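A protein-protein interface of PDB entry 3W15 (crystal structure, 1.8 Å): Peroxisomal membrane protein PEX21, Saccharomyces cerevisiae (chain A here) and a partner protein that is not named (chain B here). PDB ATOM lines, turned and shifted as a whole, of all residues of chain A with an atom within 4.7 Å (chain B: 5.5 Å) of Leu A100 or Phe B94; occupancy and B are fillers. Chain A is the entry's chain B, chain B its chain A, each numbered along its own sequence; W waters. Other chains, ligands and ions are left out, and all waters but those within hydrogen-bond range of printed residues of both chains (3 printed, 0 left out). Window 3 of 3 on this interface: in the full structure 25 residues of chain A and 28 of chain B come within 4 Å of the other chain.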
ATOM      1  N   HIS A  96     -12.303 -22.416 -12.133  1.00  0.00           N
ATOM      2  CA  HIS A  96     -12.320 -23.484 -13.137  1.00  0.00           C
ATOM      3  C   HIS A  96     -11.439 -24.634 -12.673  1.00  0.00           C
ATOM      4  O   HIS A  96     -10.465 -24.420 -11.948  1.00  0.00           O
ATOM      5  CB  HIS A  96     -11.812 -22.962 -14.478  1.00  0.00           C
ATOM      6  CG  HIS A  96     -12.609 -21.820 -15.021  1.00  0.00           C
ATOM      7  ND1 HIS A  96     -13.883 -21.973 -15.520  1.00  0.00           N
ATOM      8  CD2 HIS A  96     -12.318 -20.503 -15.130  1.00  0.00           C
ATOM      9  CE1 HIS A  96     -14.341 -20.800 -15.920  1.00  0.00           C
ATOM     10  NE2 HIS A  96     -13.411 -19.891 -15.694  1.00  0.00           N
ATOM     11  N   ASP A  98      -8.717 -27.878 -13.268  1.00  0.00           N
ATOM     12  CA  ASP A  98      -7.446 -27.953 -13.969  1.00  0.00           C
ATOM     13  C   ASP A  98      -7.636 -28.734 -15.268  1.00  0.00           C
ATOM     14  O   ASP A  98      -7.330 -29.933 -15.339  1.00  0.00           O
ATOM     15  CB  ASP A  98      -6.395 -28.612 -13.065  1.00  0.00           C
ATOM     16  CG  ASP A  98      -4.996 -28.522 -13.629  1.00  0.00           C
ATOM     17  OD1 ASP A  98      -4.797 -27.834 -14.648  1.00  0.00           O
ATOM     18  OD2 ASP A  98      -4.081 -29.147 -13.048  1.00  0.00           O
ATOM     19  N   ILE A  99      -8.153 -28.049 -16.290  1.00  0.00           N
ATOM     20  CA  ILE A  99      -8.580 -28.713 -17.539  1.00  0.00           C
ATOM     21  C   ILE A  99      -7.947 -28.075 -18.780  1.00  0.00           C
ATOM     22  O   ILE A  99      -8.273 -28.438 -19.915  1.00  0.00           O
ATOM     23  CB  ILE A  99     -10.131 -28.695 -17.692  1.00  0.00           C
ATOM     24  CG1 ILE A  99     -10.645 -27.245 -17.787  1.00  0.00           C
ATOM     25  CG2 ILE A  99     -10.795 -29.461 -16.538  1.00  0.00           C
ATOM     26  CD1 ILE A  99     -12.125 -27.099 -18.144  1.00  0.00           C
ATOM     27  N   LEU A 100      -7.042 -27.128 -18.551  1.00  0.00           N
ATOM     28  CA  LEU A 100      -6.477 -26.319 -19.620  1.00  0.00           C
ATOM     29  C   LEU A 100      -5.001 -26.095 -19.384  1.00  0.00           C
ATOM     30  O   LEU A 100      -4.606 -25.569 -18.333  1.00  0.00           O
ATOM     31  CB  LEU A 100      -7.199 -24.968 -19.694  1.00  0.00           C
ATOM     32  CG  LEU A 100      -6.791 -24.016 -20.823  1.00  0.00           C
ATOM     33  CD1 LEU A 100      -7.214 -24.585 -22.186  1.00  0.00           C
ATOM     34  CD2 LEU A 100      -7.427 -22.653 -20.593  1.00  0.00           C
ATOM     35  N   ASP A 101      -4.189 -26.502 -20.357  1.00  0.00           N
ATOM     36  CA  ASP A 101      -2.745 -26.284 -20.293  1.00  0.00           C
ATOM     37  C   ASP A 101      -2.396 -24.813 -20.442  1.00  0.00           C
ATOM     38  O   ASP A 101      -1.398 -24.360 -19.876  1.00  0.00           O
ATOM     39  CB  ASP A 101      -2.032 -27.063 -21.386  1.00  0.00           C
ATOM     40  CG  ASP A 101      -2.005 -28.551 -21.129  1.00  0.00           C
ATOM     41  OD1 ASP A 101      -2.351 -29.007 -20.020  1.00  0.00           O
ATOM     42  OD2 ASP A 101      -1.603 -29.264 -22.059  1.00  0.00           O
ATOM     43  OXT ASP A 101      -3.087 -24.059 -21.132  1.00  0.00           O
ATOM     44  N   ASN B  57     -11.720  -9.788 -23.795  1.00  0.00           N
ATOM     45  CA  ASN B  57     -12.278 -10.516 -22.663  1.00  0.00           C
ATOM     46  C   ASN B  57     -12.322  -9.610 -21.441  1.00  0.00           C
ATOM     47  O   ASN B  57     -11.649  -8.584 -21.404  1.00  0.00           O
ATOM     48  CB  ASN B  57     -11.461 -11.782 -22.365  1.00  0.00           C
ATOM     49  CG  ASN B  57     -12.277 -12.854 -21.661  1.00  0.00           C
ATOM     50  OD1 ASN B  57     -13.440 -12.645 -21.315  1.00  0.00           O
ATOM     51  ND2 ASN B  57     -11.665 -14.013 -21.443  1.00  0.00           N
ATOM     52  N   PHE B  59     -13.391  -9.952 -16.848  1.00  0.00           N
ATOM     53  CA  PHE B  59     -13.852 -10.740 -15.723  1.00  0.00           C
ATOM     54  C   PHE B  59     -14.315  -9.798 -14.625  1.00  0.00           C
ATOM     55  O   PHE B  59     -13.533  -8.997 -14.126  1.00  0.00           O
ATOM     56  CB  PHE B  59     -12.716 -11.613 -15.185  1.00  0.00           C
ATOM     57  CG  PHE B  59     -12.139 -12.572 -16.199  1.00  0.00           C
ATOM     58  CD1 PHE B  59     -11.065 -12.194 -17.003  1.00  0.00           C
ATOM     59  CD2 PHE B  59     -12.668 -13.853 -16.336  1.00  0.00           C
ATOM     60  CE1 PHE B  59     -10.520 -13.082 -17.934  1.00  0.00           C
ATOM     61  CE2 PHE B  59     -12.135 -14.755 -17.264  1.00  0.00           C
ATOM     62  CZ  PHE B  59     -11.055 -14.374 -18.061  1.00  0.00           C
ATOM     63  N   ASP B  91      -6.992 -17.340 -16.465  1.00  0.00           N
ATOM     64  CA  ASP B  91      -6.575 -17.695 -17.814  1.00  0.00           C
ATOM     65  C   ASP B  91      -7.549 -17.020 -18.775  1.00  0.00           C
ATOM     66  O   ASP B  91      -8.768 -17.219 -18.685  1.00  0.00           O
ATOM     67  CB  ASP B  91      -6.557 -19.213 -18.017  1.00  0.00           C
ATOM     68  CG  ASP B  91      -5.975 -19.611 -19.361  1.00  0.00           C
ATOM     69  OD1 ASP B  91      -6.441 -19.088 -20.390  1.00  0.00           O
ATOM     70  OD2 ASP B  91      -5.041 -20.440 -19.391  1.00  0.00           O
ATOM     71  N   THR B  92      -7.003 -16.202 -19.672  1.00  0.00           N
ATOM     72  CA  THR B  92      -7.806 -15.350 -20.566  1.00  0.00           C
ATOM     73  C   THR B  92      -8.623 -16.126 -21.609  1.00  0.00           C
ATOM     74  O   THR B  92      -9.474 -15.548 -22.306  1.00  0.00           O
ATOM     75  CB  THR B  92      -6.919 -14.289 -21.263  1.00  0.00           C
ATOM     76  OG1 THR B  92      -5.906 -14.940 -22.031  1.00  0.00           O
ATOM     77  CG2 THR B  92      -6.246 -13.398 -20.215  1.00  0.00           C
ATOM     78  N   THR B  93      -8.367 -17.430 -21.705  1.00  0.00           N
ATOM     79  CA  THR B  93      -9.121 -18.320 -22.601  1.00  0.00           C
ATOM     80  C   THR B  93     -10.523 -18.561 -22.049  1.00  0.00           C
ATOM     81  O   THR B  93     -11.488 -18.741 -22.816  1.00  0.00           O
ATOM     82  CB  THR B  93      -8.435 -19.692 -22.731  1.00  0.00           C
ATOM     83  OG1 THR B  93      -7.047 -19.509 -23.030  1.00  0.00           O
ATOM     84  CG2 THR B  93      -9.098 -20.529 -23.823  1.00  0.00           C
ATOM     85  N   PHE B  94     -10.617 -18.590 -20.720  1.00  0.00           N
ATOM     86  CA  PHE B  94     -11.859 -18.910 -20.024  1.00  0.00           C
ATOM     87  C   PHE B  94     -12.745 -17.687 -19.851  1.00  0.00           C
ATOM     88  O   PHE B  94     -12.330 -16.553 -20.117  1.00  0.00           O
ATOM     89  CB  PHE B  94     -11.571 -19.460 -18.623  1.00  0.00           C
ATOM     90  CG  PHE B  94     -11.134 -20.900 -18.586  1.00  0.00           C
ATOM     91  CD1 PHE B  94     -11.803 -21.883 -19.318  1.00  0.00           C
ATOM     92  CD2 PHE B  94     -10.082 -21.283 -17.759  1.00  0.00           C
ATOM     93  CE1 PHE B  94     -11.402 -23.211 -19.254  1.00  0.00           C
ATOM     94  CE2 PHE B  94      -9.678 -22.617 -17.686  1.00  0.00           C
ATOM     95  CZ  PHE B  94     -10.338 -23.577 -18.435  1.00  0.00           C
ATOM     96  N   LYS B  95     -13.966 -17.937 -19.384  1.00  0.00           N
ATOM     97  CA  LYS B  95     -14.894 -16.872 -19.026  1.00  0.00           C
ATOM     98  C   LYS B  95     -15.172 -16.863 -17.528  1.00  0.00           C
ATOM     99  O   LYS B  95     -15.051 -17.894 -16.858  1.00  0.00           O
ATOM    100  CB  LYS B  95     -16.223 -17.036 -19.781  1.00  0.00           C
ATOM    101  CG  LYS B  95     -16.089 -17.118 -21.313  1.00  0.00           C
ATOM    102  CD  LYS B  95     -15.475 -15.853 -21.904  1.00  0.00           C
ATOM    103  CE  LYS B  95     -15.130 -16.031 -23.385  1.00  0.00           C
ATOM    104  NZ  LYS B  95     -14.007 -16.989 -23.610  1.00  0.00           N
ATOM    105  N   GLU B  96     -15.537 -15.685 -17.029  1.00  0.00           N
ATOM    106  CA  GLU B  96     -16.245 -15.494 -15.752  1.00  0.00           C
ATOM    107  C   GLU B  96     -15.390 -15.664 -14.503  1.00  0.00           C
ATOM    108  O   GLU B  96     -15.392 -14.787 -13.634  1.00  0.00           O
ATOM    109  CB  GLU B  96     -17.518 -16.366 -15.674  1.00  0.00           C
ATOM    110  CG  GLU B  96     -18.410 -16.060 -14.472  1.00  0.00           C
ATOM    111  CD  GLU B  96     -19.784 -16.728 -14.548  1.00  0.00           C
ATOM    112  OE1 GLU B  96     -19.944 -17.707 -15.314  1.00  0.00           O
ATOM    113  OE2 GLU B  96     -20.697 -16.265 -13.838  1.00  0.00           O
ATOM    114  N   PHE B  97     -14.665 -16.781 -14.418  1.00  0.00           N
ATOM    115  CA  PHE B  97     -13.976 -17.151 -13.182  1.00  0.00           C
ATOM    116  C   PHE B  97     -12.479 -17.310 -13.354  1.00  0.00           C
ATOM    117  O   PHE B  97     -11.991 -17.526 -14.469  1.00  0.00           O
ATOM    118  CB  PHE B  97     -14.568 -18.445 -12.602  1.00  0.00           C
ATOM    119  CG  PHE B  97     -16.005 -18.317 -12.195  1.00  0.00           C
ATOM    120  CD1 PHE B  97     -16.387 -17.386 -11.237  1.00  0.00           C
ATOM    121  CD2 PHE B  97     -16.972 -19.144 -12.755  1.00  0.00           C
ATOM    122  CE1 PHE B  97     -17.728 -17.265 -10.856  1.00  0.00           C
ATOM    123  CE2 PHE B  97     -18.306 -19.045 -12.376  1.00  0.00           C
ATOM    124  CZ  PHE B  97     -18.687 -18.100 -11.430  1.00  0.00           C
ATOM    125  N   ILE B  99      -8.639 -19.219 -12.427  1.00  0.00           N
ATOM    126  CA  ILE B  99      -8.147 -20.599 -12.281  1.00  0.00           C
ATOM    127  C   ILE B  99      -7.526 -20.874 -10.897  1.00  0.00           C
ATOM    128  O   ILE B  99      -7.302 -22.033 -10.526  1.00  0.00           O
ATOM    129  CB  ILE B  99      -7.138 -20.981 -13.403  1.00  0.00           C
ATOM    130  CG1 ILE B  99      -5.908 -20.055 -13.378  1.00  0.00           C
ATOM    131  CG2 ILE B  99      -7.840 -20.959 -14.781  1.00  0.00           C
ATOM    132  CD1 ILE B  99      -4.748 -20.524 -14.224  1.00  0.00           C
HETATM  133  O   HOH W   1      -7.665 -24.478 -11.795  1.00  0.00           O
HETATM  134  O   HOH W   2      -4.103 -22.335 -17.861  1.00  0.00           O
HETATM  135  O   HOH W   3      -4.151 -21.413 -21.771  1.00  0.00           O
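Printed residues of chain B within 4 Å of His A96: Phe B94 (3.5 Å), Lys B95 (2.8 Å) and Phe B97 (3.0 Å).
Leu A100 touches three residues of chain B.
Of the printed residues of chain A, Thr B93 touches Leu A100 (3.8 Å).
Of the printed residues of chain A, Phe B97 touches His A96 (3.0 Å).
The backbone carbonyl oxygen (O) of Lys B95 is in hydrogen-bond range of a ring nitrogen (NE2) of His A96 (2.8 Å).
A ring nitrogen (NE2) of His A96 lies within hydrogen-bond range of the backbone carbonyl oxygen (O) of Phe B97, 3.0 Å away.
Hydrophobic or aromatic side chains of chain B within 4 Å of the printed part of chain A: Phe B94 and Phe B97.
Of the 5 printed residues of chain A, 3 touch a printed residue of chain B.
Among the printed residues, 7 pairs touch across the chains.
Among the printed residues, no Asp or Glu carboxylate lies within 4 Å of a Lys or Arg side-chain nitrogen of the other chain.
Phe B94 touches His A96 (CB to NE2, 3.5 Å).
Phe B94 touches Ile A99 (CZ to CG1, 3.7 Å).
Asp B91 touches Leu A100.
Leu A100 touches Thr B93.
Phe B94 touches Leu A100 (CZ to CB, 3.7 Å).
O of Phe B94 is in hydrogen-bond range of ND2 of Asn B57 (2.9 Å).
OG1 of Thr B93 lies within hydrogen-bond range of OD1 of Asp B91.
The backbone carbonyl oxygen of Thr B93 sits at hydrogen-bond distance from the side-chain amino group of Lys B95, 3.2 Å away.
Water W2 lies within hydrogen-bond range of OD2 of Asp B91 (2.6 Å) and O of Leu A100 (3.3 Å).
Water W3 lies within hydrogen-bond range of the side-chain carboxylate (OD2) of Asp B91 (2.7 Å) and the chain-end carboxylate (OXT) of Asp A101 (2.9 Å).
Water W1 bridges the backbone carbonyl oxygen of Ile B99 (2.8 Å) and the backbone carbonyl oxygen of His A96 (2.8 Å).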
